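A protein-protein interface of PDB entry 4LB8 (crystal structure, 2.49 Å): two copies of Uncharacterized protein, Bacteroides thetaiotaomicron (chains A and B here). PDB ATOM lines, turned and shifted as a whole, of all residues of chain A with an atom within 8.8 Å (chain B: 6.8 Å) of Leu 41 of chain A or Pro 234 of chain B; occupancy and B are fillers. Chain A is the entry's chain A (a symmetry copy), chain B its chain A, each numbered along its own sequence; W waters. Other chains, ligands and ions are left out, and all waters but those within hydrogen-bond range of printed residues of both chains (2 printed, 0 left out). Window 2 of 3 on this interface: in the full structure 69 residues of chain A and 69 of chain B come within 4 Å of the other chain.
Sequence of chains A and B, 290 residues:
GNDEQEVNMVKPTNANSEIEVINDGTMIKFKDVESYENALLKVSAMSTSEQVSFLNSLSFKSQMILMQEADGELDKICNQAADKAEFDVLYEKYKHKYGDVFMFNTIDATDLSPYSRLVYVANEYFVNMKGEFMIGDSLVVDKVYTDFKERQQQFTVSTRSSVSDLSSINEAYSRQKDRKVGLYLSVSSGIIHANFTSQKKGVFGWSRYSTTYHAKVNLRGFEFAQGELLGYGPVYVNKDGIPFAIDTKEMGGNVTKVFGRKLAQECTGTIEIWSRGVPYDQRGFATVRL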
ATOM      1  N   PHE A  30      -4.636 -44.243 -23.308  1.00  0.00           N
ATOM      2  CA  PHE A  30      -4.487 -43.663 -21.978  1.00  0.00           C
ATOM      3  C   PHE A  30      -4.820 -44.738 -20.961  1.00  0.00           C
ATOM      4  O   PHE A  30      -5.568 -45.668 -21.281  1.00  0.00           O
ATOM      5  CB  PHE A  30      -5.376 -42.421 -21.794  1.00  0.00           C
ATOM      6  CG  PHE A  30      -4.957 -41.269 -22.669  1.00  0.00           C
ATOM      7  CD1 PHE A  30      -3.818 -40.519 -22.368  1.00  0.00           C
ATOM      8  CD2 PHE A  30      -5.678 -40.947 -23.819  1.00  0.00           C
ATOM      9  CE1 PHE A  30      -3.417 -39.463 -23.194  1.00  0.00           C
ATOM     10  CE2 PHE A  30      -5.277 -39.887 -24.638  1.00  0.00           C
ATOM     11  CZ  PHE A  30      -4.157 -39.147 -24.316  1.00  0.00           C
ATOM     12  N   GLU A  34      -8.622 -40.003 -16.004  1.00  0.00           N
ATOM     13  CA  GLU A  34      -7.781 -39.078 -15.241  1.00  0.00           C
ATOM     14  C   GLU A  34      -6.478 -38.773 -15.998  1.00  0.00           C
ATOM     15  O   GLU A  34      -6.111 -37.600 -16.126  1.00  0.00           O
ATOM     16  CB  GLU A  34      -7.512 -39.664 -13.839  1.00  0.00           C
ATOM     17  CG  GLU A  34      -6.638 -38.819 -12.926  1.00  0.00           C
ATOM     18  CD  GLU A  34      -5.792 -39.602 -11.936  1.00  0.00           C
ATOM     19  OE1 GLU A  34      -5.299 -40.698 -12.296  1.00  0.00           O
ATOM     20  OE2 GLU A  34      -5.586 -39.096 -10.810  1.00  0.00           O
ATOM     21  N   SER A  35      -5.836 -39.819 -16.553  1.00  0.00           N
ATOM     22  CA  SER A  35      -4.618 -39.719 -17.359  1.00  0.00           C
ATOM     23  C   SER A  35      -4.867 -38.887 -18.610  1.00  0.00           C
ATOM     24  O   SER A  35      -4.101 -37.970 -18.902  1.00  0.00           O
ATOM     25  CB  SER A  35      -4.110 -41.108 -17.736  1.00  0.00           C
ATOM     26  OG  SER A  35      -3.741 -41.811 -16.562  1.00  0.00           O
ATOM     27  N   TYR A  36      -5.968 -39.180 -19.314  1.00  0.00           N
ATOM     28  CA  TYR A  36      -6.374 -38.509 -20.545  1.00  0.00           C
ATOM     29  C   TYR A  36      -6.628 -37.001 -20.280  1.00  0.00           C
ATOM     30  O   TYR A  36      -6.012 -36.161 -20.941  1.00  0.00           O
ATOM     31  CB  TYR A  36      -7.611 -39.230 -21.167  1.00  0.00           C
ATOM     32  CG  TYR A  36      -8.482 -38.331 -22.011  1.00  0.00           C
ATOM     33  CD1 TYR A  36      -8.035 -37.844 -23.238  1.00  0.00           C
ATOM     34  CD2 TYR A  36      -9.709 -37.880 -21.541  1.00  0.00           C
ATOM     35  CE1 TYR A  36      -8.788 -36.936 -23.975  1.00  0.00           C
ATOM     36  CE2 TYR A  36     -10.472 -36.975 -22.271  1.00  0.00           C
ATOM     37  CZ  TYR A  36     -10.001 -36.498 -23.483  1.00  0.00           C
ATOM     38  OH  TYR A  36     -10.759 -35.628 -24.211  1.00  0.00           O
ATOM     39  N   GLU A  37      -7.489 -36.669 -19.296  1.00  0.00           N
ATOM     40  CA  GLU A  37      -7.844 -35.287 -18.961  1.00  0.00           C
ATOM     41  C   GLU A  37      -6.618 -34.502 -18.533  1.00  0.00           C
ATOM     42  O   GLU A  37      -6.503 -33.342 -18.906  1.00  0.00           O
ATOM     43  CB  GLU A  37      -8.950 -35.227 -17.899  1.00  0.00           C
ATOM     44  CG  GLU A  37     -10.339 -35.435 -18.497  1.00  0.00           C
ATOM     45  CD  GLU A  37     -11.462 -35.742 -17.523  1.00  0.00           C
ATOM     46  OE1 GLU A  37     -11.167 -36.241 -16.412  1.00  0.00           O
ATOM     47  OE2 GLU A  37     -12.644 -35.557 -17.902  1.00  0.00           O
ATOM     48  N   ASN A  38      -5.684 -35.150 -17.801  1.00  0.00           N
ATOM     49  CA  ASN A  38      -4.427 -34.544 -17.375  1.00  0.00           C
ATOM     50  C   ASN A  38      -3.520 -34.281 -18.556  1.00  0.00           C
ATOM     51  O   ASN A  38      -3.043 -33.152 -18.690  1.00  0.00           O
ATOM     52  CB  ASN A  38      -3.722 -35.424 -16.352  1.00  0.00           C
ATOM     53  CG  ASN A  38      -4.095 -35.055 -14.945  1.00  0.00           C
ATOM     54  OD1 ASN A  38      -5.178 -35.406 -14.443  1.00  0.00           O
ATOM     55  ND2 ASN A  38      -3.243 -34.249 -14.318  1.00  0.00           N
ATOM     56  N   ALA A  39      -3.296 -35.298 -19.432  1.00  0.00           N
ATOM     57  CA  ALA A  39      -2.468 -35.151 -20.636  1.00  0.00           C
ATOM     58  C   ALA A  39      -3.039 -34.090 -21.590  1.00  0.00           C
ATOM     59  O   ALA A  39      -2.270 -33.351 -22.196  1.00  0.00           O
ATOM     60  CB  ALA A  39      -2.346 -36.474 -21.355  1.00  0.00           C
ATOM     61  N   LEU A  40      -4.379 -33.986 -21.693  1.00  0.00           N
ATOM     62  CA  LEU A  40      -5.035 -32.994 -22.544  1.00  0.00           C
ATOM     63  C   LEU A  40      -4.685 -31.548 -22.038  1.00  0.00           C
ATOM     64  O   LEU A  40      -4.249 -30.699 -22.839  1.00  0.00           O
ATOM     65  CB  LEU A  40      -6.564 -33.270 -22.563  1.00  0.00           C
ATOM     66  CG  LEU A  40      -7.470 -32.460 -23.529  1.00  0.00           C
ATOM     67  CD1 LEU A  40      -7.241 -32.830 -24.988  1.00  0.00           C
ATOM     68  CD2 LEU A  40      -8.926 -32.652 -23.162  1.00  0.00           C
ATOM     69  N   LEU A  41      -4.794 -31.317 -20.704  1.00  0.00           N
ATOM     70  CA  LEU A  41      -4.489 -30.047 -20.044  1.00  0.00           C
ATOM     71  C   LEU A  41      -3.023 -29.673 -20.227  1.00  0.00           C
ATOM     72  O   LEU A  41      -2.735 -28.560 -20.673  1.00  0.00           O
ATOM     73  CB  LEU A  41      -4.832 -30.112 -18.534  1.00  0.00           C
ATOM     74  CG  LEU A  41      -4.490 -28.847 -17.712  1.00  0.00           C
ATOM     75  CD1 LEU A  41      -5.382 -27.665 -18.139  1.00  0.00           C
ATOM     76  CD2 LEU A  41      -4.639 -29.115 -16.244  1.00  0.00           C
ATOM     77  N   LYS A  42      -2.097 -30.603 -19.880  1.00  0.00           N
ATOM     78  CA  LYS A  42      -0.649 -30.382 -19.999  1.00  0.00           C
ATOM     79  C   LYS A  42      -0.256 -30.131 -21.463  1.00  0.00           C
ATOM     80  O   LYS A  42       0.397 -29.128 -21.726  1.00  0.00           O
ATOM     81  CB  LYS A  42       0.169 -31.536 -19.403  1.00  0.00           C
ATOM     82  CG  LYS A  42      -0.111 -31.877 -17.931  1.00  0.00           C
ATOM     83  CD  LYS A  42       0.621 -31.006 -16.915  1.00  0.00           C
ATOM     84  CE  LYS A  42       0.274 -31.393 -15.490  1.00  0.00           C
ATOM     85  NZ  LYS A  42       1.108 -30.662 -14.490  1.00  0.00           N
ATOM     86  N   VAL A  43      -0.709 -30.972 -22.411  1.00  0.00           N
ATOM     87  CA  VAL A  43      -0.379 -30.794 -23.832  1.00  0.00           C
ATOM     88  C   VAL A  43      -1.057 -29.535 -24.420  1.00  0.00           C
ATOM     89  O   VAL A  43      -0.364 -28.771 -25.084  1.00  0.00           O
ATOM     90  CB  VAL A  43      -0.669 -32.051 -24.685  1.00  0.00           C
ATOM     91  CG1 VAL A  43      -0.378 -31.809 -26.169  1.00  0.00           C
ATOM     92  CG2 VAL A  43       0.154 -33.221 -24.176  1.00  0.00           C
ATOM     93  N   SER A  44      -2.360 -29.276 -24.148  1.00  0.00           N
ATOM     94  CA  SER A  44      -2.996 -28.078 -24.720  1.00  0.00           C
ATOM     95  C   SER A  44      -2.403 -26.761 -24.192  1.00  0.00           C
ATOM     96  O   SER A  44      -2.610 -25.746 -24.842  1.00  0.00           O
ATOM     97  CB  SER A  44      -4.510 -28.081 -24.530  1.00  0.00           C
ATOM     98  OG  SER A  44      -4.896 -27.769 -23.205  1.00  0.00           O
ATOM     99  N   ALA A  45      -1.614 -26.785 -23.084  1.00  0.00           N
ATOM    100  CA  ALA A  45      -1.017 -25.583 -22.468  1.00  0.00           C
ATOM    101  C   ALA A  45       0.382 -25.244 -22.998  1.00  0.00           C
ATOM    102  O   ALA A  45       0.902 -24.136 -22.761  1.00  0.00           O
ATOM    103  CB  ALA A  45      -0.964 -25.746 -20.974  1.00  0.00           C
ATOM    104  N   MET A  46       0.968 -26.189 -23.736  1.00  0.00           N
ATOM    105  CA  MET A  46       2.265 -26.060 -24.392  1.00  0.00           C
ATOM    106  C   MET A  46       2.196 -25.145 -25.612  1.00  0.00           C
ATOM    107  O   MET A  46       1.110 -24.856 -26.125  1.00  0.00           O
ATOM    108  CB  MET A  46       2.723 -27.445 -24.856  1.00  0.00           C
ATOM    109  CG  MET A  46       3.016 -28.406 -23.721  1.00  0.00           C
ATOM    110  SD  MET A  46       3.688 -30.039 -24.476  1.00  0.00           S
ATOM    111  CE  MET A  46       3.546 -31.200 -22.880  1.00  0.00           C
ATOM    112  N   GLN A  51       4.292 -28.867 -28.529  1.00  0.00           N
ATOM    113  CA  GLN A  51       3.298 -29.893 -28.827  1.00  0.00           C
ATOM    114  C   GLN A  51       3.753 -30.787 -29.965  1.00  0.00           C
ATOM    115  O   GLN A  51       3.628 -32.006 -29.849  1.00  0.00           O
ATOM    116  CB  GLN A  51       1.959 -29.270 -29.190  1.00  0.00           C
ATOM    117  CG  GLN A  51       1.282 -28.581 -28.046  1.00  0.00           C
ATOM    118  CD  GLN A  51       0.239 -27.668 -28.569  1.00  0.00           C
ATOM    119  OE1 GLN A  51       0.097 -27.487 -29.781  1.00  0.00           O
ATOM    120  NE2 GLN A  51      -0.518 -27.067 -27.667  1.00  0.00           N
ATOM    121  N   ALA A 122      -9.761 -29.731 -28.792  1.00  0.00           N
ATOM    122  CA  ALA A 122      -8.438 -29.990 -28.198  1.00  0.00           C
ATOM    123  C   ALA A 122      -8.046 -31.470 -28.320  1.00  0.00           C
ATOM    124  O   ALA A 122      -6.873 -31.768 -28.279  1.00  0.00           O
ATOM    125  CB  ALA A 122      -8.385 -29.524 -26.753  1.00  0.00           C
ATOM    126  N   ASN A 123      -8.999 -32.364 -28.609  1.00  0.00           N
ATOM    127  CA  ASN A 123      -8.713 -33.790 -28.810  1.00  0.00           C
ATOM    128  C   ASN A 123      -7.858 -34.061 -30.073  1.00  0.00           C
ATOM    129  O   ASN A 123      -7.340 -35.171 -30.213  1.00  0.00           O
ATOM    130  CB  ASN A 123      -9.996 -34.595 -28.866  1.00  0.00           C
ATOM    131  CG  ASN A 123     -10.542 -34.888 -27.506  1.00  0.00           C
ATOM    132  OD1 ASN A 123      -9.810 -34.917 -26.535  1.00  0.00           O
ATOM    133  ND2 ASN A 123     -11.833 -35.154 -27.390  1.00  0.00           N
ATOM    134  N   TYR A 125      -4.919 -33.241 -30.690  1.00  0.00           N
ATOM    135  CA  TYR A 125      -3.591 -33.640 -30.242  1.00  0.00           C
ATOM    136  C   TYR A 125      -3.451 -35.157 -30.123  1.00  0.00           C
ATOM    137  O   TYR A 125      -2.349 -35.666 -30.275  1.00  0.00           O
ATOM    138  CB  TYR A 125      -3.278 -33.010 -28.867  1.00  0.00           C
ATOM    139  CG  TYR A 125      -3.324 -31.499 -28.859  1.00  0.00           C
ATOM    140  CD1 TYR A 125      -2.452 -30.752 -29.642  1.00  0.00           C
ATOM    141  CD2 TYR A 125      -4.189 -30.813 -28.014  1.00  0.00           C
ATOM    142  CE1 TYR A 125      -2.522 -29.362 -29.673  1.00  0.00           C
ATOM    143  CE2 TYR A 125      -4.239 -29.422 -28.005  1.00  0.00           C
ATOM    144  CZ  TYR A 125      -3.407 -28.699 -28.841  1.00  0.00           C
ATOM    145  OH  TYR A 125      -3.453 -27.329 -28.843  1.00  0.00           O
ATOM    146  N   PHE A 126      -4.540 -35.881 -29.814  1.00  0.00           N
ATOM    147  CA  PHE A 126      -4.400 -37.303 -29.563  1.00  0.00           C
ATOM    148  C   PHE A 126      -5.147 -38.197 -30.563  1.00  0.00           C
ATOM    149  O   PHE A 126      -4.708 -39.336 -30.734  1.00  0.00           O
ATOM    150  CB  PHE A 126      -4.831 -37.632 -28.129  1.00  0.00           C
ATOM    151  CG  PHE A 126      -4.230 -36.785 -27.023  1.00  0.00           C
ATOM    152  CD1 PHE A 126      -2.855 -36.711 -26.848  1.00  0.00           C
ATOM    153  CD2 PHE A 126      -5.045 -36.112 -26.121  1.00  0.00           C
ATOM    154  CE1 PHE A 126      -2.299 -35.953 -25.799  1.00  0.00           C
ATOM    155  CE2 PHE A 126      -4.492 -35.371 -25.066  1.00  0.00           C
ATOM    156  CZ  PHE A 126      -3.123 -35.284 -24.919  1.00  0.00           C
ATOM    157  N   PHE B 224     -10.917 -21.647 -14.821  1.00  0.00           N
ATOM    158  CA  PHE B 224     -10.094 -21.389 -15.991  1.00  0.00           C
ATOM    159  C   PHE B 224      -8.849 -22.245 -15.995  1.00  0.00           C
ATOM    160  O   PHE B 224      -8.171 -22.375 -14.965  1.00  0.00           O
ATOM    161  CB  PHE B 224      -9.721 -19.912 -16.055  1.00  0.00           C
ATOM    162  CG  PHE B 224      -8.839 -19.478 -17.202  1.00  0.00           C
ATOM    163  CD1 PHE B 224      -9.243 -19.663 -18.522  1.00  0.00           C
ATOM    164  CD2 PHE B 224      -7.652 -18.792 -16.966  1.00  0.00           C
ATOM    165  CE1 PHE B 224      -8.454 -19.204 -19.575  1.00  0.00           C
ATOM    166  CE2 PHE B 224      -6.859 -18.340 -18.024  1.00  0.00           C
ATOM    167  CZ  PHE B 224      -7.266 -18.544 -19.320  1.00  0.00           C
ATOM    168  N   ALA B 225      -8.539 -22.817 -17.176  1.00  0.00           N
ATOM    169  CA  ALA B 225      -7.341 -23.622 -17.396  1.00  0.00           C
ATOM    170  C   ALA B 225      -6.202 -22.668 -17.686  1.00  0.00           C
ATOM    171  O   ALA B 225      -5.926 -22.344 -18.840  1.00  0.00           O
ATOM    172  CB  ALA B 225      -7.556 -24.605 -18.535  1.00  0.00           C
ATOM    173  N   GLN B 226      -5.598 -22.141 -16.599  1.00  0.00           N
ATOM    174  CA  GLN B 226      -4.508 -21.178 -16.631  1.00  0.00           C
ATOM    175  C   GLN B 226      -3.228 -21.842 -17.149  1.00  0.00           C
ATOM    176  O   GLN B 226      -2.874 -22.900 -16.653  1.00  0.00           O
ATOM    177  CB  GLN B 226      -4.315 -20.607 -15.219  1.00  0.00           C
ATOM    178  CG  GLN B 226      -3.231 -19.571 -15.086  1.00  0.00           C
ATOM    179  CD  GLN B 226      -3.156 -19.048 -13.681  1.00  0.00           C
ATOM    180  OE1 GLN B 226      -4.002 -18.262 -13.253  1.00  0.00           O
ATOM    181  NE2 GLN B 226      -2.151 -19.491 -12.923  1.00  0.00           N
ATOM    182  N   GLY B 227      -2.553 -21.214 -18.111  1.00  0.00           N
ATOM    183  CA  GLY B 227      -1.308 -21.715 -18.695  1.00  0.00           C
ATOM    184  C   GLY B 227      -0.128 -21.650 -17.748  1.00  0.00           C
ATOM    185  O   GLY B 227      -0.245 -21.058 -16.674  1.00  0.00           O
ATOM    186  N   GLU B 228       1.020 -22.264 -18.125  1.00  0.00           N
ATOM    187  CA  GLU B 228       2.216 -22.297 -17.271  1.00  0.00           C
ATOM    188  C   GLU B 228       2.820 -20.895 -17.113  1.00  0.00           C
ATOM    189  O   GLU B 228       3.076 -20.189 -18.090  1.00  0.00           O
ATOM    190  CB  GLU B 228       3.267 -23.289 -17.791  1.00  0.00           C
ATOM    191  N   LEU B 229       2.994 -20.489 -15.861  1.00  0.00           N
ATOM    192  CA  LEU B 229       3.516 -19.184 -15.487  1.00  0.00           C
ATOM    193  C   LEU B 229       4.522 -19.376 -14.364  1.00  0.00           C
ATOM    194  O   LEU B 229       4.185 -20.002 -13.345  1.00  0.00           O
ATOM    195  CB  LEU B 229       2.335 -18.292 -15.055  1.00  0.00           C
ATOM    196  CG  LEU B 229       2.633 -16.968 -14.365  1.00  0.00           C
ATOM    197  CD1 LEU B 229       2.773 -15.832 -15.370  1.00  0.00           C
ATOM    198  CD2 LEU B 229       1.534 -16.636 -13.431  1.00  0.00           C
ATOM    199  N   TYR B 232       4.860 -22.727 -12.683  1.00  0.00           N
ATOM    200  CA  TYR B 232       3.661 -23.208 -11.974  1.00  0.00           C
ATOM    201  C   TYR B 232       2.510 -23.379 -13.004  1.00  0.00           C
ATOM    202  O   TYR B 232       2.373 -22.566 -13.930  1.00  0.00           O
ATOM    203  CB  TYR B 232       3.281 -22.278 -10.791  1.00  0.00           C
ATOM    204  CG  TYR B 232       1.861 -22.415 -10.261  1.00  0.00           C
ATOM    205  CD1 TYR B 232       1.434 -23.586  -9.637  1.00  0.00           C
ATOM    206  CD2 TYR B 232       0.965 -21.352 -10.329  1.00  0.00           C
ATOM    207  CE1 TYR B 232       0.137 -23.711  -9.138  1.00  0.00           C
ATOM    208  CE2 TYR B 232      -0.334 -21.467  -9.831  1.00  0.00           C
ATOM    209  CZ  TYR B 232      -0.739 -22.645  -9.228  1.00  0.00           C
ATOM    210  OH  TYR B 232      -2.023 -22.766  -8.749  1.00  0.00           O
ATOM    211  N   GLY B 233       1.736 -24.459 -12.850  1.00  0.00           N
ATOM    212  CA  GLY B 233       0.645 -24.810 -13.752  1.00  0.00           C
ATOM    213  C   GLY B 233       1.095 -25.624 -14.963  1.00  0.00           C
ATOM    214  O   GLY B 233       2.252 -26.052 -15.011  1.00  0.00           O
ATOM    215  N   PRO B 234       0.241 -25.859 -15.994  1.00  0.00           N
ATOM    216  CA  PRO B 234      -1.162 -25.434 -16.152  1.00  0.00           C
ATOM    217  C   PRO B 234      -2.034 -25.910 -15.002  1.00  0.00           C
ATOM    218  O   PRO B 234      -1.869 -27.018 -14.507  1.00  0.00           O
ATOM    219  CB  PRO B 234      -1.569 -26.063 -17.491  1.00  0.00           C
ATOM    220  CG  PRO B 234      -0.614 -27.202 -17.683  1.00  0.00           C
ATOM    221  CD  PRO B 234       0.671 -26.659 -17.158  1.00  0.00           C
ATOM    222  N   VAL B 235      -2.913 -25.041 -14.538  1.00  0.00           N
ATOM    223  CA  VAL B 235      -3.765 -25.346 -13.401  1.00  0.00           C
ATOM    224  C   VAL B 235      -5.172 -24.715 -13.580  1.00  0.00           C
ATOM    225  O   VAL B 235      -5.320 -23.665 -14.228  1.00  0.00           O
ATOM    226  CB  VAL B 235      -3.058 -24.869 -12.087  1.00  0.00           C
ATOM    227  CG1 VAL B 235      -2.838 -23.342 -12.064  1.00  0.00           C
ATOM    228  CG2 VAL B 235      -3.782 -25.359 -10.836  1.00  0.00           C
ATOM    229  N   TYR B 236      -6.192 -25.365 -12.975  1.00  0.00           N
ATOM    230  CA  TYR B 236      -7.555 -24.863 -12.950  1.00  0.00           C
ATOM    231  C   TYR B 236      -7.675 -23.849 -11.842  1.00  0.00           C
ATOM    232  O   TYR B 236      -7.491 -24.179 -10.676  1.00  0.00           O
ATOM    233  CB  TYR B 236      -8.571 -25.990 -12.794  1.00  0.00           C
ATOM    234  CG  TYR B 236      -8.687 -26.847 -14.033  1.00  0.00           C
ATOM    235  CD1 TYR B 236      -9.180 -26.322 -15.227  1.00  0.00           C
ATOM    236  CD2 TYR B 236      -8.275 -28.176 -14.023  1.00  0.00           C
ATOM    237  CE1 TYR B 236      -9.241 -27.092 -16.380  1.00  0.00           C
ATOM    238  CE2 TYR B 236      -8.353 -28.966 -15.168  1.00  0.00           C
ATOM    239  CZ  TYR B 236      -8.854 -28.424 -16.340  1.00  0.00           C
ATOM    240  OH  TYR B 236      -8.949 -29.218 -17.453  1.00  0.00           O
ATOM    241  N   VAL B 258      -7.821 -26.463 -23.877  1.00  0.00           N
ATOM    242  CA  VAL B 258      -8.705 -26.778 -22.770  1.00  0.00           C
ATOM    243  C   VAL B 258      -8.933 -25.388 -22.198  1.00  0.00           C
ATOM    244  O   VAL B 258      -7.960 -24.724 -21.813  1.00  0.00           O
ATOM    245  CB  VAL B 258      -8.074 -27.768 -21.750  1.00  0.00           C
ATOM    246  CG1 VAL B 258      -8.902 -27.835 -20.470  1.00  0.00           C
ATOM    247  CG2 VAL B 258      -7.909 -29.145 -22.349  1.00  0.00           C
HETATM  248  O   HOH W   1      -7.791 -32.019 -16.900  1.00  0.00           O
HETATM  249  O   HOH W   2      -5.011 -25.457 -22.095  1.00  0.00           O
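OG of Ser 44 of chain A sits at hydrogen-bond distance from N of Val 258 of chain B (3.3 Å).
O of Leu 40 of chain A lies within hydrogen-bond range of OG of Ser 44 of chain A, at 3.0 Å.
The backbone carbonyl oxygen (O) of Leu 41 of chain A lies within hydrogen-bond range of the side-chain hydroxyl (OG) of Ser 44 of chain A, 3.4 Å away.
Among the printed residues, merely in contact across the chains: Leu 40 of chain A with Val 258 of chain B (3.5 Å), Ala 45 of chain A with Pro 234 of chain B (3.5 Å), Leu 41 of chain A with Ala 225 of chain B (3.8 Å), Leu 41 of chain A with Tyr 236 of chain B (3.9 Å), Leu 41 of chain A with Pro 234 of chain B (3.9 Å) and Lys 42 of chain A with Pro 234 of chain B (3.9 Å).
Leu 41 of chain A touches just these residues of chain B: Ala 225 (3.8 Å), Pro 234 (3.9 Å) and Tyr 236 (3.9 Å).
No residue of chain A comes within 4 Å of Gly 233 of chain B.
Val 235 of chain B touches none of the printed residues of chain A.
Printed residues of chain B within 4 Å of Ser 44 of chain A: Val 258.
Printed residues of chain B within 4 Å of Leu 40 of chain A: Val 258.
Printed residues of chain A within 4 Å of Tyr 236 of chain B: Leu 41 (3.9 Å).
Val 43 of chain A touches none of the printed residues of chain B.
The nearest residue of chain B that does not touch Leu 41 of chain A is Val 258 of chain B (4.1 Å).
The nearest printed residue of chain B that does not touch Ser 44 of chain A is Ala 225 of chain B (6.2 Å).
Of the 12 printed residues of chain B, 4 touch a printed residue of chain A.
Hydrophobic or aromatic side chains of chain B that line the printed part of chain A: Ala 225, Pro 234, Tyr 236 and Val 258.
Of the 19 printed residues of chain A, 5 touch a printed residue of chain B.
Printed residues of chain A that touch a printed residue of chain B: Leu 40, Leu 41, Lys 42, Ser 44 and Ala 45.
Along chain A the printed residues that touch a printed residue of chain B span positions 40 to 45.
Among the printed residues, no Asp or Glu carboxylate lies within 4 Å of a Lys or Arg side-chain nitrogen of the other chain.
No position is printed for both chains.
Of the 7 pairs that touch across the chains among the printed residues, none has its exchanged pair printed and touching as well.
Water W2 bridges OG of Ser 44 of chain A and O of Val 258 of chain B.
Water W1 lies within hydrogen-bond range of the backbone carbonyl oxygen of Glu 37 of chain A and the side-chain hydroxyl of Tyr 236 of chain B.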
